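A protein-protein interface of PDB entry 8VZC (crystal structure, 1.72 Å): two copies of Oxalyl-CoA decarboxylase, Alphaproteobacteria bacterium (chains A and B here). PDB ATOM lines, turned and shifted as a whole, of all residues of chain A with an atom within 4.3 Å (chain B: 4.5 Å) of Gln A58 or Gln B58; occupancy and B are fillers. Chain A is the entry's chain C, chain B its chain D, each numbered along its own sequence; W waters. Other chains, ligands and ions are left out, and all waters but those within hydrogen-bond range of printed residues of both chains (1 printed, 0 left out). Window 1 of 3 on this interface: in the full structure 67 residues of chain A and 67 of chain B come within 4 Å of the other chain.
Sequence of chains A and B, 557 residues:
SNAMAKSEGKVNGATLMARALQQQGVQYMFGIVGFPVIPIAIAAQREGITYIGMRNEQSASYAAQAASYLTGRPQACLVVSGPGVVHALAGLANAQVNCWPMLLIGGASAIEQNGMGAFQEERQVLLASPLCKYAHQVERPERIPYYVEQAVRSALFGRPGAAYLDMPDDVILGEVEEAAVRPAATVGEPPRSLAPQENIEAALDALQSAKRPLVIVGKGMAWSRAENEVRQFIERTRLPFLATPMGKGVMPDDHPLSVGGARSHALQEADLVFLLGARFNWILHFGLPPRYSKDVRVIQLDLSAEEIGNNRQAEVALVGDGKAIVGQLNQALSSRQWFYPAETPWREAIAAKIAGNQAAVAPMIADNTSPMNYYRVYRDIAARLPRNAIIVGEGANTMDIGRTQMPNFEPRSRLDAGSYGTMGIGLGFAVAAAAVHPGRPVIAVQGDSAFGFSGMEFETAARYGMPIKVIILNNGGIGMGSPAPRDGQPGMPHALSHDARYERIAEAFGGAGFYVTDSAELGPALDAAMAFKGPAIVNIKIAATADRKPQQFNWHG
The side-chain amide nitrogen (ND2) of Asn A56 lies within hydrogen-bond range of the side-chain amide oxygen (OE1) of Gln B58 (2.8 Å). ND2 of Asn B56 sits at hydrogen-bond distance from OE1 of Gln A58 (2.6 Å). The side-chain hydroxyl (OH) of Tyr A62 sits at hydrogen-bond distance from a ring nitrogen (NE2) of His B87, at 2.7 Å. OH of Tyr B62 lies within hydrogen-bond range of NE2 of His A87, 2.6 Å away.
OD1 of Asn A56 sits at hydrogen-bond distance from N of Gln A58 (2.9 Å). The side-chain carboxylate (OE1) of Glu A57 sits at hydrogen-bond distance from a ring nitrogen (ND1) of His A87, at 2.9 Å. The side-chain hydroxyl (OG) of Ser A61 is in hydrogen-bond range of the backbone carbonyl oxygen (O) of Gln A58 (3.0 Å). The backbone NH of Gln B58 lies within hydrogen-bond range of the side-chain amide oxygen of Asn B56, at 2.9 Å. The side-chain carboxylate of Glu B57 lies within hydrogen-bond range of a ring nitrogen (ND1) of His B87, 2.8 Å away. The side-chain hydroxyl (OG) of Ser B61 sits at hydrogen-bond distance from the backbone carbonyl oxygen (O) of Gln B58, 2.9 Å away.
Among the printed residues, pairs that only touch across the chains: Gln A58 with Gln B58 (3.8 Å), Gln A58 with His B87 (3.3 Å), His A87 with Gln B58 (3.3 Å), His A87 with Ala B90 (3.5 Å) and Ala A90 with His B87 (3.6 Å).
Of the printed residues of chain B, Asn A56 touches Gln B58. Glu A57 touches none of the printed residues of chain B. Of the printed residues of chain B, Tyr A62 touches His B87. Of the printed residues of chain B, Ala A90 touches His B87 (3.6 Å). Of the printed residues of chain A, Gln B58 touches Asn A56 (2.8 Å), Gln A58 (3.8 Å) and His A87 (3.3 Å). The nearest printed residue of chain B that does not touch Gln A58 is Glu B57 (5.3 Å). The nearest printed residue of chain A that does not touch Ala B90 is Gln A58 (6.9 Å).
Hydrophobic or aromatic side chains of chain B that line the printed part of chain A: Tyr B62, His B87 and Ala B90. Hydrophobic or aromatic side chains of chain A that line the printed part of chain B: Tyr A62, His A87 and Ala A90. Among the printed residues, no Asp or Glu carboxylate lies within 4 Å of a Lys or Arg side-chain nitrogen of the other chain.
Asn A56 touches Gln B58, and with the chains exchanged Gln A58 touches Asn B56. Gln B58 touches its own counterpart, Gln A58. Tyr A62 touches His B87, and with the chains exchanged His A87 touches Tyr B62. His A87 touches Ala B90, and with the chains exchanged Ala A90 touches His B87. Positions printed for both chains: 56, 57, 58, 59, 60, 61, 62, 87 and 90.
Water W1 lies within hydrogen-bond range of the side-chain amide nitrogen (NE2) of Gln A58 (3.0 Å), the side-chain amide nitrogen (NE2) of Gln B58 (3.0 Å) and the backbone carbonyl oxygen (O) of His A87 (3.2 Å).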
ATOM      1  N   ASN A  56     -28.361 -11.936   5.106  1.00  0.00           N
ATOM      2  CA  ASN A  56     -28.024 -12.041   3.683  1.00  0.00           C
ATOM      3  C   ASN A  56     -28.391 -13.448   3.196  1.00  0.00           C
ATOM      4  O   ASN A  56     -28.118 -14.436   3.893  1.00  0.00           O
ATOM      5  CB  ASN A  56     -26.541 -11.741   3.447  1.00  0.00           C
ATOM      6  CG  ASN A  56     -26.229 -11.461   1.948  1.00  0.00           C
ATOM      7  OD1 ASN A  56     -26.505 -12.313   1.074  1.00  0.00           O
ATOM      8  ND2 ASN A  56     -25.662 -10.296   1.668  1.00  0.00           N
ATOM      9  N   GLU A  57     -29.037 -13.532   2.012  1.00  0.00           N
ATOM     10  CA  GLU A  57     -29.428 -14.830   1.445  1.00  0.00           C
ATOM     11  C   GLU A  57     -28.238 -15.747   1.269  1.00  0.00           C
ATOM     12  O   GLU A  57     -28.392 -16.966   1.237  1.00  0.00           O
ATOM     13  CB  GLU A  57     -30.094 -14.675   0.058  1.00  0.00           C
ATOM     14  CG  GLU A  57     -31.451 -14.015   0.056  1.00  0.00           C
ATOM     15  CD  GLU A  57     -31.355 -12.509   0.051  1.00  0.00           C
ATOM     16  OE1 GLU A  57     -30.231 -11.957  -0.056  1.00  0.00           O
ATOM     17  OE2 GLU A  57     -32.426 -11.879   0.140  1.00  0.00           O
ATOM     18  N   GLN A  58     -27.062 -15.184   1.044  1.00  0.00           N
ATOM     19  CA  GLN A  58     -25.877 -16.019   0.905  1.00  0.00           C
ATOM     20  C   GLN A  58     -25.708 -16.896   2.152  1.00  0.00           C
ATOM     21  O   GLN A  58     -25.552 -18.125   2.066  1.00  0.00           O
ATOM     22  CB  GLN A  58     -24.678 -15.096   0.683  1.00  0.00           C
ATOM     23  CG  GLN A  58     -23.408 -15.736   0.221  1.00  0.00           C
ATOM     24  CD  GLN A  58     -22.272 -14.740   0.196  1.00  0.00           C
ATOM     25  OE1 GLN A  58     -21.541 -14.589   1.185  1.00  0.00           O
ATOM     26  NE2 GLN A  58     -22.114 -14.047  -0.927  1.00  0.00           N
ATOM     27  N   SER A  59     -25.827 -16.285   3.319  1.00  0.00           N
ATOM     28  CA  SER A  59     -25.716 -17.041   4.569  1.00  0.00           C
ATOM     29  C   SER A  59     -26.923 -17.939   4.792  1.00  0.00           C
ATOM     30  O   SER A  59     -26.795 -19.027   5.372  1.00  0.00           O
ATOM     31  CB  SER A  59     -25.549 -16.093   5.744  1.00  0.00           C
ATOM     32  OG  SER A  59     -24.247 -15.546   5.731  1.00  0.00           O
ATOM     33  N   ALA A  60     -28.109 -17.484   4.385  1.00  0.00           N
ATOM     34  CA  ALA A  60     -29.290 -18.326   4.515  1.00  0.00           C
ATOM     35  C   ALA A  60     -29.156 -19.607   3.690  1.00  0.00           C
ATOM     36  O   ALA A  60     -29.559 -20.693   4.136  1.00  0.00           O
ATOM     37  CB  ALA A  60     -30.533 -17.545   4.086  1.00  0.00           C
ATOM     38  N   SER A  61     -28.599 -19.505   2.474  1.00  0.00           N
ATOM     39  CA  SER A  61     -28.520 -20.689   1.625  1.00  0.00           C
ATOM     40  C   SER A  61     -27.452 -21.644   2.133  1.00  0.00           C
ATOM     41  O   SER A  61     -27.554 -22.865   1.924  1.00  0.00           O
ATOM     42  CB  SER A  61     -28.251 -20.289   0.149  1.00  0.00           C
ATOM     43  OG  SER A  61     -26.945 -19.729  -0.002  1.00  0.00           O
ATOM     44  N   TYR A  62     -26.448 -21.108   2.832  1.00  0.00           N
ATOM     45  CA  TYR A  62     -25.475 -21.955   3.517  1.00  0.00           C
ATOM     46  C   TYR A  62     -26.076 -22.601   4.766  1.00  0.00           C
ATOM     47  O   TYR A  62     -25.838 -23.788   5.033  1.00  0.00           O
ATOM     48  CB  TYR A  62     -24.236 -21.137   3.870  1.00  0.00           C
ATOM     49  CG  TYR A  62     -23.412 -20.706   2.656  1.00  0.00           C
ATOM     50  CD1 TYR A  62     -23.216 -21.567   1.568  1.00  0.00           C
ATOM     51  CD2 TYR A  62     -22.774 -19.460   2.646  1.00  0.00           C
ATOM     52  CE1 TYR A  62     -22.439 -21.170   0.464  1.00  0.00           C
ATOM     53  CE2 TYR A  62     -21.981 -19.065   1.565  1.00  0.00           C
ATOM     54  CZ  TYR A  62     -21.826 -19.923   0.487  1.00  0.00           C
ATOM     55  OH  TYR A  62     -21.071 -19.506  -0.581  1.00  0.00           O
ATOM     56  N   HIS A  87     -28.412 -14.136  -5.128  1.00  0.00           N
ATOM     57  CA  HIS A  87     -27.618 -14.240  -3.889  1.00  0.00           C
ATOM     58  C   HIS A  87     -27.569 -15.685  -3.379  1.00  0.00           C
ATOM     59  O   HIS A  87     -26.528 -16.142  -2.882  1.00  0.00           O
ATOM     60  CB  HIS A  87     -28.180 -13.342  -2.783  1.00  0.00           C
ATOM     61  CG  HIS A  87     -27.936 -11.869  -2.969  1.00  0.00           C
ATOM     62  ND1 HIS A  87     -28.371 -10.930  -2.058  1.00  0.00           N
ATOM     63  CD2 HIS A  87     -27.344 -11.169  -3.970  1.00  0.00           C
ATOM     64  CE1 HIS A  87     -28.049  -9.716  -2.477  1.00  0.00           C
ATOM     65  NE2 HIS A  87     -27.429  -9.829  -3.640  1.00  0.00           N
ATOM     66  N   ALA A  90     -24.997 -19.038  -4.356  1.00  0.00           N
ATOM     67  CA  ALA A  90     -23.878 -19.394  -3.476  1.00  0.00           C
ATOM     68  C   ALA A  90     -24.071 -20.750  -2.806  1.00  0.00           C
ATOM     69  O   ALA A  90     -23.207 -21.632  -2.883  1.00  0.00           O
ATOM     70  CB  ALA A  90     -23.711 -18.320  -2.393  1.00  0.00           C
ATOM     71  N   ASN B  56     -16.997  -8.978   1.154  1.00  0.00           N
ATOM     72  CA  ASN B  56     -17.750 -10.044   0.498  1.00  0.00           C
ATOM     73  C   ASN B  56     -17.791  -9.716  -0.996  1.00  0.00           C
ATOM     74  O   ASN B  56     -18.014  -8.565  -1.361  1.00  0.00           O
ATOM     75  CB  ASN B  56     -19.167 -10.175   1.092  1.00  0.00           C
ATOM     76  CG  ASN B  56     -19.905 -11.481   0.650  1.00  0.00           C
ATOM     77  OD1 ASN B  56     -20.097 -11.744  -0.551  1.00  0.00           O
ATOM     78  ND2 ASN B  56     -20.319 -12.304   1.635  1.00  0.00           N
ATOM     79  N   GLU B  57     -17.546 -10.721  -1.849  1.00  0.00           N
ATOM     80  CA  GLU B  57     -17.583 -10.479  -3.304  1.00  0.00           C
ATOM     81  C   GLU B  57     -18.924  -9.941  -3.766  1.00  0.00           C
ATOM     82  O   GLU B  57     -19.004  -9.296  -4.815  1.00  0.00           O
ATOM     83  CB  GLU B  57     -17.316 -11.757  -4.108  1.00  0.00           C
ATOM     84  CG  GLU B  57     -15.953 -12.349  -3.923  1.00  0.00           C
ATOM     85  CD  GLU B  57     -15.880 -13.235  -2.681  1.00  0.00           C
ATOM     86  OE1 GLU B  57     -16.906 -13.465  -1.996  1.00  0.00           O
ATOM     87  OE2 GLU B  57     -14.765 -13.677  -2.400  1.00  0.00           O
ATOM     88  N   GLN B  58     -20.001 -10.276  -3.077  1.00  0.00           N
ATOM     89  CA  GLN B  58     -21.294  -9.699  -3.429  1.00  0.00           C
ATOM     90  C   GLN B  58     -21.212  -8.169  -3.501  1.00  0.00           C
ATOM     91  O   GLN B  58     -21.577  -7.549  -4.528  1.00  0.00           O
ATOM     92  CB  GLN B  58     -22.315 -10.176  -2.396  1.00  0.00           C
ATOM     93  CG  GLN B  58     -23.731  -9.930  -2.783  1.00  0.00           C
ATOM     94  CD  GLN B  58     -24.680 -10.335  -1.686  1.00  0.00           C
ATOM     95  OE1 GLN B  58     -25.166  -9.491  -0.951  1.00  0.00           O
ATOM     96  NE2 GLN B  58     -24.966 -11.624  -1.589  1.00  0.00           N
ATOM     97  N   SER B  59     -20.645  -7.548  -2.459  1.00  0.00           N
ATOM     98  CA  SER B  59     -20.454  -6.092  -2.434  1.00  0.00           C
ATOM     99  C   SER B  59     -19.405  -5.626  -3.445  1.00  0.00           C
ATOM    100  O   SER B  59     -19.518  -4.523  -3.996  1.00  0.00           O
ATOM    101  CB  SER B  59     -20.054  -5.620  -1.030  1.00  0.00           C
ATOM    102  OG  SER B  59     -21.187  -5.422  -0.199  1.00  0.00           O
ATOM    103  N   ALA B  60     -18.330  -6.404  -3.644  1.00  0.00           N
ATOM    104  CA  ALA B  60     -17.334  -6.002  -4.628  1.00  0.00           C
ATOM    105  C   ALA B  60     -17.936  -5.953  -6.028  1.00  0.00           C
ATOM    106  O   ALA B  60     -17.560  -5.101  -6.857  1.00  0.00           O
ATOM    107  CB  ALA B  60     -16.148  -6.959  -4.593  1.00  0.00           C
ATOM    108  N   SER B  61     -18.813  -6.911  -6.341  1.00  0.00           N
ATOM    109  CA  SER B  61     -19.347  -6.920  -7.701  1.00  0.00           C
ATOM    110  C   SER B  61     -20.326  -5.768  -7.894  1.00  0.00           C
ATOM    111  O   SER B  61     -20.428  -5.216  -9.006  1.00  0.00           O
ATOM    112  CB  SER B  61     -19.988  -8.282  -8.006  1.00  0.00           C
ATOM    113  OG  SER B  61     -21.146  -8.514  -7.207  1.00  0.00           O
ATOM    114  N   TYR B  62     -21.024  -5.374  -6.814  1.00  0.00           N
ATOM    115  CA  TYR B  62     -21.889  -4.190  -6.869  1.00  0.00           C
ATOM    116  C   TYR B  62     -21.064  -2.911  -6.962  1.00  0.00           C
ATOM    117  O   TYR B  62     -21.415  -1.985  -7.724  1.00  0.00           O
ATOM    118  CB  TYR B  62     -22.811  -4.144  -5.647  1.00  0.00           C
ATOM    119  CG  TYR B  62     -23.873  -5.214  -5.623  1.00  0.00           C
ATOM    120  CD1 TYR B  62     -24.508  -5.626  -6.809  1.00  0.00           C
ATOM    121  CD2 TYR B  62     -24.253  -5.817  -4.413  1.00  0.00           C
ATOM    122  CE1 TYR B  62     -25.468  -6.620  -6.804  1.00  0.00           C
ATOM    123  CE2 TYR B  62     -25.244  -6.813  -4.396  1.00  0.00           C
ATOM    124  CZ  TYR B  62     -25.854  -7.194  -5.582  1.00  0.00           C
ATOM    125  OH  TYR B  62     -26.796  -8.175  -5.592  1.00  0.00           O
ATOM    126  N   HIS B  87     -20.424 -16.070  -5.732  1.00  0.00           N
ATOM    127  CA  HIS B  87     -20.787 -14.877  -4.950  1.00  0.00           C
ATOM    128  C   HIS B  87     -20.940 -13.631  -5.822  1.00  0.00           C
ATOM    129  O   HIS B  87     -21.829 -12.808  -5.576  1.00  0.00           O
ATOM    130  CB  HIS B  87     -19.739 -14.577  -3.882  1.00  0.00           C
ATOM    131  CG  HIS B  87     -19.780 -15.512  -2.699  1.00  0.00           C
ATOM    132  ND1 HIS B  87     -18.933 -15.373  -1.627  1.00  0.00           N
ATOM    133  CD2 HIS B  87     -20.545 -16.596  -2.443  1.00  0.00           C
ATOM    134  CE1 HIS B  87     -19.184 -16.327  -0.740  1.00  0.00           C
ATOM    135  NE2 HIS B  87     -20.156 -17.090  -1.212  1.00  0.00           N
ATOM    136  N   ALA B  90     -24.184 -12.130  -8.258  1.00  0.00           N
ATOM    137  CA  ALA B  90     -25.036 -11.015  -7.823  1.00  0.00           C
ATOM    138  C   ALA B  90     -24.796  -9.736  -8.641  1.00  0.00           C
ATOM    139  O   ALA B  90     -25.734  -9.154  -9.204  1.00  0.00           O
ATOM    140  CB  ALA B  90     -24.802 -10.733  -6.333  1.00  0.00           C
HETATM  141  O   HOH W   1     -24.083 -14.030  -3.172  1.00  0.00           O
